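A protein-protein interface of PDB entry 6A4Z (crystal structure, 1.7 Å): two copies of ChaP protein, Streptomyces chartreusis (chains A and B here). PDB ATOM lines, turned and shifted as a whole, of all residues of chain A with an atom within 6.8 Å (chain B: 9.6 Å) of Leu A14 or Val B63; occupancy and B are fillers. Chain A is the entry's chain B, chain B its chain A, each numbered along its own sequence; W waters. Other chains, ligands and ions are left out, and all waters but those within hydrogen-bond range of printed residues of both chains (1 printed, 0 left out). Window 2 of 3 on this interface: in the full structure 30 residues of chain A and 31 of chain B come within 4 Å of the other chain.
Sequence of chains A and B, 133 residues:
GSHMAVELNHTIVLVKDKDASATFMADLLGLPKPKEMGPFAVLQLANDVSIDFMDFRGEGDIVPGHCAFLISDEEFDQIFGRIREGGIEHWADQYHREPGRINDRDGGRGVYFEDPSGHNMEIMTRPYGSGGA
The backbone carbonyl oxygen (O) of His B66 sits at hydrogen-bond distance from the backbone NH (N) of Ile A12 (3.0 Å).
Water W1 lies within hydrogen-bond range of the backbone carbonyl oxygen of Ile A12 and the backbone NH of His B66.
A ring nitrogen (ND1) of His B66 is in hydrogen-bond range of the backbone carbonyl oxygen (O) of Asn B120. The backbone carbonyl oxygen (O) of Leu A14 lies within hydrogen-bond range of a ring nitrogen (NE2) of His A119 (2.7 Å). The backbone carbonyl oxygen of Val A15 lies within hydrogen-bond range of the backbone NH of Phe A56 (2.7 Å).
Of chain B, only Val B63 comes within 4 Å of Leu A14. Of chain A, only Leu A14 (3.7 Å), Phe A56 (3.9 Å) and Glu A59 (3.5 Å) come within 4 Å of Val B63. No residue of chain B comes within 4 Å of Val A15. Of the printed residues of chain B, Phe A56 touches Val B63. Printed residues of chain B within 4 Å of Ile A12: His B66 (3.0 Å). Met A54 touches none of the printed residues of chain B.
Among the printed residues, merely in contact across the chains: Leu A14 with Val B63 (3.7 Å), Phe A56 with Val B63 (3.9 Å) and Glu A59 with Val B63 (3.5 Å).
Of the 20 printed residues of chain B, 2 touch a printed residue of chain A. Printed residues of chain B that touch a printed residue of chain A: Val B63 and His B66. Hydrophobic or aromatic side chains of chain A that line the printed part of chain B: Ile A12, Leu A14 and Phe A56. Along chain A the printed residues that touch a printed residue of chain B span positions 12 to 59.
Leu A14 touches Val B63, but with the chains exchanged Val A63 does not touch Leu B14 (4.02 Å). Phe A56 touches Val B63, but with the chains exchanged Val A63 does not touch Phe B56 (4.1 Å). Glu A59 touches Val B63, but with the chains exchanged Val A63 does not touch Glu B59 (5.9 Å). Positions printed for both chains: 12, 13, 14, 15, 16, 56, 59, 62, 63, 115, 117 and 119. Of the 4 pairs that touch across the chains among the printed residues, none has its exchanged pair printed and touching as well.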
ATOM      1  N   ILE A  12     -37.208 -12.105  31.025  1.00  0.00           N
ATOM      2  CA  ILE A  12     -36.229 -13.089  30.571  1.00  0.00           C
ATOM      3  C   ILE A  12     -34.872 -12.716  31.134  1.00  0.00           C
ATOM      4  O   ILE A  12     -34.494 -11.539  31.153  1.00  0.00           O
ATOM      5  CB  ILE A  12     -36.187 -13.169  29.030  1.00  0.00           C
ATOM      6  CG1 ILE A  12     -37.414 -13.925  28.505  1.00  0.00           C
ATOM      7  CG2 ILE A  12     -34.895 -13.863  28.575  1.00  0.00           C
ATOM      8  CD1 ILE A  12     -37.573 -13.916  26.963  1.00  0.00           C
ATOM      9  N   VAL A  13     -34.134 -13.722  31.608  1.00  0.00           N
ATOM     10  CA  VAL A  13     -32.735 -13.569  31.969  1.00  0.00           C
ATOM     11  C   VAL A  13     -31.927 -14.496  31.074  1.00  0.00           C
ATOM     12  O   VAL A  13     -32.165 -15.711  31.053  1.00  0.00           O
ATOM     13  CB  VAL A  13     -32.487 -13.869  33.453  1.00  0.00           C
ATOM     14  CG1 VAL A  13     -30.986 -13.909  33.729  1.00  0.00           C
ATOM     15  CG2 VAL A  13     -33.150 -12.796  34.297  1.00  0.00           C
ATOM     16  N   LEU A  14     -30.995 -13.920  30.322  1.00  0.00           N
ATOM     17  CA  LEU A  14     -30.177 -14.667  29.382  1.00  0.00           C
ATOM     18  C   LEU A  14     -28.956 -15.236  30.089  1.00  0.00           C
ATOM     19  O   LEU A  14     -28.218 -14.493  30.747  1.00  0.00           O
ATOM     20  CB  LEU A  14     -29.726 -13.752  28.244  1.00  0.00           C
ATOM     21  CG  LEU A  14     -30.875 -13.166  27.432  1.00  0.00           C
ATOM     22  CD1 LEU A  14     -30.335 -12.109  26.500  1.00  0.00           C
ATOM     23  CD2 LEU A  14     -31.574 -14.275  26.670  1.00  0.00           C
ATOM     24  N   VAL A  15     -28.719 -16.541  29.921  1.00  0.00           N
ATOM     25  CA  VAL A  15     -27.617 -17.223  30.592  1.00  0.00           C
ATOM     26  C   VAL A  15     -26.967 -18.222  29.636  1.00  0.00           C
ATOM     27  O   VAL A  15     -27.527 -18.588  28.601  1.00  0.00           O
ATOM     28  CB  VAL A  15     -28.089 -17.937  31.876  1.00  0.00           C
ATOM     29  CG1 VAL A  15     -28.535 -16.930  32.930  1.00  0.00           C
ATOM     30  CG2 VAL A  15     -29.226 -18.861  31.563  1.00  0.00           C
ATOM     31  N   LYS A  16     -25.777 -18.701  30.021  1.00  0.00           N
ATOM     32  CA  LYS A  16     -25.121 -19.745  29.234  1.00  0.00           C
ATOM     33  C   LYS A  16     -25.876 -21.066  29.294  1.00  0.00           C
ATOM     34  O   LYS A  16     -25.856 -21.838  28.326  1.00  0.00           O
ATOM     35  CB  LYS A  16     -23.679 -19.956  29.714  1.00  0.00           C
ATOM     36  CG  LYS A  16     -22.750 -18.788  29.472  1.00  0.00           C
ATOM     37  CD  LYS A  16     -22.460 -18.640  27.985  1.00  0.00           C
ATOM     38  CE  LYS A  16     -21.322 -17.669  27.732  1.00  0.00           C
ATOM     39  NZ  LYS A  16     -21.058 -17.520  26.277  1.00  0.00           N
ATOM     40  N   ASP A  17     -26.528 -21.362  30.417  1.00  0.00           N
ATOM     41  CA  ASP A  17     -27.191 -22.654  30.586  1.00  0.00           C
ATOM     42  C   ASP A  17     -28.426 -22.423  31.454  1.00  0.00           C
ATOM     43  O   ASP A  17     -28.314 -22.289  32.676  1.00  0.00           O
ATOM     44  CB  ASP A  17     -26.227 -23.664  31.199  1.00  0.00           C
ATOM     45  CG  ASP A  17     -26.866 -25.023  31.465  1.00  0.00           C
ATOM     46  OD1 ASP A  17     -28.089 -25.182  31.310  1.00  0.00           O
ATOM     47  OD2 ASP A  17     -26.123 -25.951  31.826  1.00  0.00           O
ATOM     48  N   SER A  21     -28.582 -22.406  35.646  1.00  0.00           N
ATOM     49  CA  SER A  21     -28.851 -21.181  36.391  1.00  0.00           C
ATOM     50  C   SER A  21     -30.157 -21.276  37.165  1.00  0.00           C
ATOM     51  O   SER A  21     -30.216 -20.884  38.338  1.00  0.00           O
ATOM     52  CB  SER A  21     -28.860 -19.973  35.446  1.00  0.00           C
ATOM     53  OG  SER A  21     -27.534 -19.606  35.087  1.00  0.00           O
ATOM     54  N   ASP A  52     -37.630 -15.939  33.642  1.00  0.00           N
ATOM     55  CA  ASP A  52     -37.631 -16.960  32.603  1.00  0.00           C
ATOM     56  C   ASP A  52     -36.214 -17.055  32.058  1.00  0.00           C
ATOM     57  O   ASP A  52     -35.803 -16.260  31.204  1.00  0.00           O
ATOM     58  CB  ASP A  52     -38.652 -16.619  31.524  1.00  0.00           C
ATOM     59  CG  ASP A  52     -40.082 -16.538  32.075  1.00  0.00           C
ATOM     60  OD1 ASP A  52     -40.299 -16.846  33.268  1.00  0.00           O
ATOM     61  OD2 ASP A  52     -41.004 -16.164  31.323  1.00  0.00           O
ATOM     62  N   PHE A  53     -35.467 -18.031  32.561  1.00  0.00           N
ATOM     63  CA  PHE A  53     -34.099 -18.231  32.106  1.00  0.00           C
ATOM     64  C   PHE A  53     -34.085 -18.793  30.695  1.00  0.00           C
ATOM     65  O   PHE A  53     -34.836 -19.718  30.372  1.00  0.00           O
ATOM     66  CB  PHE A  53     -33.356 -19.166  33.058  1.00  0.00           C
ATOM     67  CG  PHE A  53     -33.000 -18.519  34.364  1.00  0.00           C
ATOM     68  CD1 PHE A  53     -31.871 -17.717  34.463  1.00  0.00           C
ATOM     69  CD2 PHE A  53     -33.810 -18.675  35.475  1.00  0.00           C
ATOM     70  CE1 PHE A  53     -31.539 -17.101  35.651  1.00  0.00           C
ATOM     71  CE2 PHE A  53     -33.479 -18.056  36.682  1.00  0.00           C
ATOM     72  CZ  PHE A  53     -32.329 -17.277  36.766  1.00  0.00           C
ATOM     73  N   MET A  54     -33.237 -18.213  29.853  1.00  0.00           N
ATOM     74  CA  MET A  54     -33.126 -18.628  28.476  1.00  0.00           C
ATOM     75  C   MET A  54     -31.659 -18.760  28.084  1.00  0.00           C
ATOM     76  O   MET A  54     -30.831 -17.925  28.486  1.00  0.00           O
ATOM     77  CB  MET A  54     -33.838 -17.622  27.570  1.00  0.00           C
ATOM     78  CG  MET A  54     -33.696 -17.918  26.110  1.00  0.00           C
ATOM     79  SD  MET A  54     -34.581 -16.524  25.060  1.00  0.00           S
ATOM     80  CE  MET A  54     -35.005 -17.616  23.500  1.00  0.00           C
ATOM     81  N   ASP A  55     -31.345 -19.807  27.317  1.00  0.00           N
ATOM     82  CA  ASP A  55     -30.003 -19.978  26.768  1.00  0.00           C
ATOM     83  C   ASP A  55     -29.640 -18.816  25.855  1.00  0.00           C
ATOM     84  O   ASP A  55     -30.423 -18.426  24.983  1.00  0.00           O
ATOM     85  CB  ASP A  55     -29.908 -21.290  25.980  1.00  0.00           C
ATOM     86  CG  ASP A  55     -29.989 -22.518  26.867  1.00  0.00           C
ATOM     87  OD1 ASP A  55     -29.682 -22.409  28.064  1.00  0.00           O
ATOM     88  OD2 ASP A  55     -30.374 -23.594  26.363  1.00  0.00           O
ATOM     89  N   PHE A  56     -28.451 -18.260  26.046  1.00  0.00           N
ATOM     90  CA  PHE A  56     -27.946 -17.207  25.169  1.00  0.00           C
ATOM     91  C   PHE A  56     -26.497 -17.591  24.908  1.00  0.00           C
ATOM     92  O   PHE A  56     -25.634 -17.409  25.773  1.00  0.00           O
ATOM     93  CB  PHE A  56     -28.065 -15.844  25.833  1.00  0.00           C
ATOM     94  CG  PHE A  56     -27.542 -14.718  25.006  1.00  0.00           C
ATOM     95  CD1 PHE A  56     -28.161 -14.369  23.817  1.00  0.00           C
ATOM     96  CD2 PHE A  56     -26.426 -14.011  25.410  1.00  0.00           C
ATOM     97  CE1 PHE A  56     -27.676 -13.322  23.051  1.00  0.00           C
ATOM     98  CE2 PHE A  56     -25.938 -12.965  24.652  1.00  0.00           C
ATOM     99  CZ  PHE A  56     -26.562 -12.624  23.470  1.00  0.00           C
ATOM    100  N   GLU A  59     -22.379 -14.096  21.156  1.00  0.00           N
ATOM    101  CA  GLU A  59     -21.551 -13.091  21.831  1.00  0.00           C
ATOM    102  C   GLU A  59     -20.319 -13.813  22.395  1.00  0.00           C
ATOM    103  O   GLU A  59     -19.863 -14.821  21.842  1.00  0.00           O
ATOM    104  CB  GLU A  59     -22.391 -12.363  22.860  1.00  0.00           C
ATOM    105  CG  GLU A  59     -22.312 -10.851  22.820  1.00  0.00           C
ATOM    106  CD  GLU A  59     -23.545 -10.232  22.203  1.00  0.00           C
ATOM    107  OE1 GLU A  59     -24.322 -10.978  21.574  1.00  0.00           O
ATOM    108  OE2 GLU A  59     -23.743  -9.009  22.351  1.00  0.00           O
ATOM    109  N   ILE A  62     -21.671 -13.349  28.957  1.00  0.00           N
ATOM    110  CA  ILE A  62     -22.906 -12.696  29.369  1.00  0.00           C
ATOM    111  C   ILE A  62     -22.574 -11.343  29.987  1.00  0.00           C
ATOM    112  O   ILE A  62     -21.665 -11.233  30.822  1.00  0.00           O
ATOM    113  CB  ILE A  62     -23.660 -13.587  30.367  1.00  0.00           C
ATOM    114  CG1 ILE A  62     -23.977 -14.962  29.765  1.00  0.00           C
ATOM    115  CG2 ILE A  62     -24.901 -12.893  30.857  1.00  0.00           C
ATOM    116  CD1 ILE A  62     -24.928 -14.927  28.597  1.00  0.00           C
ATOM    117  N   VAL A  63     -23.304 -10.305  29.585  1.00  0.00           N
ATOM    118  CA  VAL A  63     -23.218  -9.026  30.290  1.00  0.00           C
ATOM    119  C   VAL A  63     -24.025  -9.173  31.575  1.00  0.00           C
ATOM    120  O   VAL A  63     -25.229  -9.450  31.514  1.00  0.00           O
ATOM    121  CB  VAL A  63     -23.736  -7.859  29.437  1.00  0.00           C
ATOM    122  CG1 VAL A  63     -23.754  -6.574  30.255  1.00  0.00           C
ATOM    123  CG2 VAL A  63     -22.894  -7.699  28.177  1.00  0.00           C
ATOM    124  N   ASP A 115     -24.917 -16.023  39.950  1.00  0.00           N
ATOM    125  CA  ASP A 115     -25.360 -17.274  39.354  1.00  0.00           C
ATOM    126  C   ASP A 115     -24.250 -17.828  38.470  1.00  0.00           C
ATOM    127  O   ASP A 115     -23.217 -17.183  38.280  1.00  0.00           O
ATOM    128  CB  ASP A 115     -26.650 -17.047  38.565  1.00  0.00           C
ATOM    129  CG  ASP A 115     -26.379 -16.688  37.125  1.00  0.00           C
ATOM    130  OD1 ASP A 115     -25.651 -15.704  36.897  1.00  0.00           O
ATOM    131  OD2 ASP A 115     -26.860 -17.407  36.232  1.00  0.00           O
ATOM    132  N   SER A 117     -23.747 -17.895  35.417  1.00  0.00           N
ATOM    133  CA  SER A 117     -23.365 -17.040  34.295  1.00  0.00           C
ATOM    134  C   SER A 117     -22.825 -15.675  34.715  1.00  0.00           C
ATOM    135  O   SER A 117     -22.458 -14.878  33.845  1.00  0.00           O
ATOM    136  CB  SER A 117     -24.559 -16.839  33.351  1.00  0.00           C
ATOM    137  OG  SER A 117     -24.746 -17.976  32.537  1.00  0.00           O
ATOM    138  N   HIS A 119     -24.389 -13.239  36.652  1.00  0.00           N
ATOM    139  CA  HIS A 119     -25.358 -12.211  37.004  1.00  0.00           C
ATOM    140  C   HIS A 119     -25.233 -11.833  38.473  1.00  0.00           C
ATOM    141  O   HIS A 119     -24.894 -12.656  39.323  1.00  0.00           O
ATOM    142  CB  HIS A 119     -26.767 -12.696  36.711  1.00  0.00           C
ATOM    143  CG  HIS A 119     -27.032 -12.875  35.256  1.00  0.00           C
ATOM    144  ND1 HIS A 119     -26.943 -11.830  34.363  1.00  0.00           N
ATOM    145  CD2 HIS A 119     -27.397 -13.961  34.536  1.00  0.00           C
ATOM    146  CE1 HIS A 119     -27.244 -12.264  33.151  1.00  0.00           C
ATOM    147  NE2 HIS A 119     -27.516 -13.554  33.228  1.00  0.00           N
ATOM    148  N   THR B  11     -35.172  -5.556  39.265  1.00  0.00           N
ATOM    149  CA  THR B  11     -34.268  -6.084  38.265  1.00  0.00           C
ATOM    150  C   THR B  11     -33.830  -4.921  37.390  1.00  0.00           C
ATOM    151  O   THR B  11     -34.581  -3.963  37.190  1.00  0.00           O
ATOM    152  CB  THR B  11     -34.905  -7.203  37.439  1.00  0.00           C
ATOM    153  OG1 THR B  11     -33.905  -7.793  36.596  1.00  0.00           O
ATOM    154  CG2 THR B  11     -36.039  -6.661  36.576  1.00  0.00           C
ATOM    155  N   ILE B  12     -32.593  -4.986  36.918  1.00  0.00           N
ATOM    156  CA  ILE B  12     -32.028  -3.929  36.085  1.00  0.00           C
ATOM    157  C   ILE B  12     -32.312  -4.225  34.623  1.00  0.00           C
ATOM    158  O   ILE B  12     -32.176  -5.365  34.171  1.00  0.00           O
ATOM    159  CB  ILE B  12     -30.515  -3.797  36.321  1.00  0.00           C
ATOM    160  CG1 ILE B  12     -30.236  -3.113  37.657  1.00  0.00           C
ATOM    161  CG2 ILE B  12     -29.849  -3.028  35.186  1.00  0.00           C
ATOM    162  CD1 ILE B  12     -28.756  -3.074  37.996  1.00  0.00           C
ATOM    163  N   VAL B  13     -32.697  -3.197  33.875  1.00  0.00           N
ATOM    164  CA  VAL B  13     -32.773  -3.277  32.424  1.00  0.00           C
ATOM    165  C   VAL B  13     -31.822  -2.226  31.864  1.00  0.00           C
ATOM    166  O   VAL B  13     -31.955  -1.034  32.169  1.00  0.00           O
ATOM    167  CB  VAL B  13     -34.201  -3.069  31.905  1.00  0.00           C
ATOM    168  CG1 VAL B  13     -34.187  -2.974  30.388  1.00  0.00           C
ATOM    169  CG2 VAL B  13     -35.099  -4.219  32.355  1.00  0.00           C
ATOM    170  N   LEU B  14     -30.856  -2.669  31.068  1.00  0.00           N
ATOM    171  CA  LEU B  14     -29.857  -1.787  30.483  1.00  0.00           C
ATOM    172  C   LEU B  14     -30.396  -1.201  29.181  1.00  0.00           C
ATOM    173  O   LEU B  14     -30.923  -1.938  28.342  1.00  0.00           O
ATOM    174  CB  LEU B  14     -28.561  -2.557  30.231  1.00  0.00           C
ATOM    175  CG  LEU B  14     -27.889  -3.081  31.498  1.00  0.00           C
ATOM    176  CD1 LEU B  14     -26.750  -4.049  31.162  1.00  0.00           C
ATOM    177  CD2 LEU B  14     -27.366  -1.901  32.311  1.00  0.00           C
ATOM    178  N   VAL B  15     -30.273   0.121  29.022  1.00  0.00           N
ATOM    179  CA  VAL B  15     -30.802   0.832  27.862  1.00  0.00           C
ATOM    180  C   VAL B  15     -29.805   1.901  27.419  1.00  0.00           C
ATOM    181  O   VAL B  15     -28.827   2.206  28.108  1.00  0.00           O
ATOM    182  CB  VAL B  15     -32.182   1.465  28.151  1.00  0.00           C
ATOM    183  CG1 VAL B  15     -33.233   0.369  28.374  1.00  0.00           C
ATOM    184  CG2 VAL B  15     -32.091   2.386  29.361  1.00  0.00           C
ATOM    185  N   LYS B  16     -30.050   2.449  26.222  1.00  0.00           N
ATOM    186  CA  LYS B  16     -29.235   3.559  25.737  1.00  0.00           C
ATOM    187  C   LYS B  16     -29.487   4.837  26.531  1.00  0.00           C
ATOM    188  O   LYS B  16     -28.565   5.637  26.720  1.00  0.00           O
ATOM    189  CB  LYS B  16     -29.512   3.804  24.253  1.00  0.00           C
ATOM    190  CG  LYS B  16     -29.149   2.634  23.347  1.00  0.00           C
ATOM    191  CD  LYS B  16     -27.648   2.425  23.249  1.00  0.00           C
ATOM    192  CE  LYS B  16     -27.320   1.422  22.151  1.00  0.00           C
ATOM    193  NZ  LYS B  16     -25.861   1.140  22.049  1.00  0.00           N
ATOM    194  N   PHE B  56     -26.541   1.776  29.583  1.00  0.00           N
ATOM    195  CA  PHE B  56     -25.546   0.760  29.254  1.00  0.00           C
ATOM    196  C   PHE B  56     -24.197   1.416  28.964  1.00  0.00           C
ATOM    197  O   PHE B  56     -24.087   2.281  28.084  1.00  0.00           O
ATOM    198  CB  PHE B  56     -26.012  -0.080  28.070  1.00  0.00           C
ATOM    199  CG  PHE B  56     -25.008  -1.115  27.625  1.00  0.00           C
ATOM    200  CD1 PHE B  56     -24.593  -2.110  28.494  1.00  0.00           C
ATOM    201  CD2 PHE B  56     -24.519  -1.117  26.328  1.00  0.00           C
ATOM    202  CE1 PHE B  56     -23.673  -3.061  28.098  1.00  0.00           C
ATOM    203  CE2 PHE B  56     -23.605  -2.073  25.920  1.00  0.00           C
ATOM    204  CZ  PHE B  56     -23.182  -3.047  26.807  1.00  0.00           C
ATOM    205  N   GLU B  59     -20.128  -1.767  25.257  1.00  0.00           N
ATOM    206  CA  GLU B  59     -20.314  -1.759  23.813  1.00  0.00           C
ATOM    207  C   GLU B  59     -20.894  -3.110  23.416  1.00  0.00           C
ATOM    208  O   GLU B  59     -20.681  -4.109  24.107  1.00  0.00           O
ATOM    209  CB  GLU B  59     -18.989  -1.503  23.079  1.00  0.00           C
ATOM    210  CG  GLU B  59     -17.952  -2.595  23.284  1.00  0.00           C
ATOM    211  CD  GLU B  59     -16.723  -2.413  22.409  1.00  0.00           C
ATOM    212  OE1 GLU B  59     -16.781  -1.609  21.454  1.00  0.00           O
ATOM    213  OE2 GLU B  59     -15.697  -3.076  22.677  1.00  0.00           O
ATOM    214  N   GLY B  60     -21.640  -3.153  22.314  1.00  0.00           N
ATOM    215  CA  GLY B  60     -21.977  -2.018  21.477  1.00  0.00           C
ATOM    216  C   GLY B  60     -23.479  -1.838  21.450  1.00  0.00           C
ATOM    217  O   GLY B  60     -24.007  -0.842  21.944  1.00  0.00           O
ATOM    218  N   ASP B  61     -24.179  -2.823  20.894  1.00  0.00           N
ATOM    219  CA  ASP B  61     -25.631  -2.776  20.839  1.00  0.00           C
ATOM    220  C   ASP B  61     -26.229  -3.430  22.079  1.00  0.00           C
ATOM    221  O   ASP B  61     -25.637  -4.326  22.684  1.00  0.00           O
ATOM    222  CB  ASP B  61     -26.150  -3.488  19.586  1.00  0.00           C
ATOM    223  CG  ASP B  61     -25.744  -2.790  18.302  1.00  0.00           C
ATOM    224  OD1 ASP B  61     -24.524  -2.697  18.045  1.00  0.00           O
ATOM    225  OD2 ASP B  61     -26.635  -2.353  17.543  1.00  0.00           O
ATOM    226  N   ILE B  62     -27.409  -2.943  22.464  1.00  0.00           N
ATOM    227  CA  ILE B  62     -28.201  -3.589  23.502  1.00  0.00           C
ATOM    228  C   ILE B  62     -28.671  -4.946  22.996  1.00  0.00           C
ATOM    229  O   ILE B  62     -29.240  -5.055  21.900  1.00  0.00           O
ATOM    230  CB  ILE B  62     -29.408  -2.714  23.871  1.00  0.00           C
ATOM    231  CG1 ILE B  62     -28.983  -1.294  24.248  1.00  0.00           C
ATOM    232  CG2 ILE B  62     -30.198  -3.353  25.002  1.00  0.00           C
ATOM    233  CD1 ILE B  62     -28.132  -1.209  25.456  1.00  0.00           C
ATOM    234  N   VAL B  63     -28.459  -5.986  23.792  1.00  0.00           N
ATOM    235  CA  VAL B  63     -29.104  -7.260  23.497  1.00  0.00           C
ATOM    236  C   VAL B  63     -30.535  -7.148  24.008  1.00  0.00           C
ATOM    237  O   VAL B  63     -30.732  -6.927  25.211  1.00  0.00           O
ATOM    238  CB  VAL B  63     -28.354  -8.444  24.125  1.00  0.00           C
ATOM    239  CG1 VAL B  63     -29.149  -9.720  23.936  1.00  0.00           C
ATOM    240  CG2 VAL B  63     -26.972  -8.581  23.499  1.00  0.00           C
ATOM    241  N   PRO B  64     -31.548  -7.256  23.146  1.00  0.00           N
ATOM    242  CA  PRO B  64     -32.929  -7.017  23.593  1.00  0.00           C
ATOM    243  C   PRO B  64     -33.371  -8.050  24.614  1.00  0.00           C
ATOM    244  O   PRO B  64     -33.171  -9.256  24.434  1.00  0.00           O
ATOM    245  CB  PRO B  64     -33.748  -7.119  22.302  1.00  0.00           C
ATOM    246  CG  PRO B  64     -32.756  -6.931  21.195  1.00  0.00           C
ATOM    247  CD  PRO B  64     -31.472  -7.502  21.695  1.00  0.00           C
ATOM    248  N   GLY B  65     -33.942  -7.563  25.709  1.00  0.00           N
ATOM    249  CA  GLY B  65     -34.558  -8.402  26.709  1.00  0.00           C
ATOM    250  C   GLY B  65     -36.056  -8.518  26.501  1.00  0.00           C
ATOM    251  O   GLY B  65     -36.590  -8.196  25.433  1.00  0.00           O
ATOM    252  N   HIS B  66     -36.746  -8.948  27.555  1.00  0.00           N
ATOM    253  CA  HIS B  66     -38.196  -9.153  27.487  1.00  0.00           C
ATOM    254  C   HIS B  66     -38.786  -8.914  28.866  1.00  0.00           C
ATOM    255  O   HIS B  66     -38.364  -9.547  29.839  1.00  0.00           O
ATOM    256  CB  HIS B  66     -38.520 -10.565  27.008  1.00  0.00           C
ATOM    257  CG  HIS B  66     -39.982 -10.884  26.990  1.00  0.00           C
ATOM    258  ND1 HIS B  66     -40.905 -10.081  26.353  1.00  0.00           N
ATOM    259  CD2 HIS B  66     -40.681 -11.919  27.516  1.00  0.00           C
ATOM    260  CE1 HIS B  66     -42.109 -10.613  26.479  1.00  0.00           C
ATOM    261  NE2 HIS B  66     -42.002 -11.730  27.173  1.00  0.00           N
ATOM    262  N   ASP B 115     -39.517  -0.804  23.743  1.00  0.00           N
ATOM    263  CA  ASP B 115     -39.084   0.421  24.372  1.00  0.00           C
ATOM    264  C   ASP B 115     -38.090   1.115  23.440  1.00  0.00           C
ATOM    265  O   ASP B 115     -37.695   0.543  22.419  1.00  0.00           O
ATOM    266  CB  ASP B 115     -38.478   0.102  25.735  1.00  0.00           C
ATOM    267  CG  ASP B 115     -36.991  -0.146  25.657  1.00  0.00           C
ATOM    268  OD1 ASP B 115     -36.577  -1.073  24.928  1.00  0.00           O
ATOM    269  OD2 ASP B 115     -36.248   0.612  26.302  1.00  0.00           O
ATOM    270  N   SER B 117     -35.005   1.466  23.407  1.00  0.00           N
ATOM    271  CA  SER B 117     -33.771   0.727  23.150  1.00  0.00           C
ATOM    272  C   SER B 117     -34.007  -0.614  22.479  1.00  0.00           C
ATOM    273  O   SER B 117     -33.045  -1.346  22.240  1.00  0.00           O
ATOM    274  CB  SER B 117     -32.973   0.509  24.447  1.00  0.00           C
ATOM    275  OG  SER B 117     -32.254   1.669  24.803  1.00  0.00           O
ATOM    276  N   GLY B 118     -35.251  -0.961  22.166  1.00  0.00           N
ATOM    277  CA  GLY B 118     -35.515  -2.175  21.425  1.00  0.00           C
ATOM    278  C   GLY B 118     -35.833  -3.400  22.250  1.00  0.00           C
ATOM    279  O   GLY B 118     -35.910  -4.499  21.683  1.00  0.00           O
ATOM    280  N   HIS B 119     -35.999  -3.264  23.565  1.00  0.00           N
ATOM    281  CA  HIS B 119     -36.403  -4.411  24.369  1.00  0.00           C
ATOM    282  C   HIS B 119     -37.813  -4.832  23.980  1.00  0.00           C
ATOM    283  O   HIS B 119     -38.648  -4.004  23.615  1.00  0.00           O
ATOM    284  CB  HIS B 119     -36.350  -4.086  25.862  1.00  0.00           C
ATOM    285  CG  HIS B 119     -34.964  -3.844  26.380  1.00  0.00           C
ATOM    286  ND1 HIS B 119     -33.985  -4.814  26.356  1.00  0.00           N
ATOM    287  CD2 HIS B 119     -34.384  -2.736  26.900  1.00  0.00           C
ATOM    288  CE1 HIS B 119     -32.871  -4.326  26.874  1.00  0.00           C
ATOM    289  NE2 HIS B 119     -33.085  -3.065  27.208  1.00  0.00           N
ATOM    290  N   ASN B 120     -38.072  -6.131  24.055  1.00  0.00           N
ATOM    291  CA  ASN B 120     -39.360  -6.687  23.643  1.00  0.00           C
ATOM    292  C   ASN B 120     -40.336  -6.613  24.812  1.00  0.00           C
ATOM    293  O   ASN B 120     -40.242  -7.395  25.761  1.00  0.00           O
ATOM    294  CB  ASN B 120     -39.188  -8.123  23.170  1.00  0.00           C
ATOM    295  CG  ASN B 120     -40.391  -8.623  22.427  1.00  0.00           C
ATOM    296  OD1 ASN B 120     -41.294  -7.850  22.091  1.00  0.00           O
ATOM    297  ND2 ASN B 120     -40.406  -9.909  22.142  1.00  0.00           N
HETATM  298  O   HOH W   1     -35.034  -9.445  29.790  1.00  0.00           O
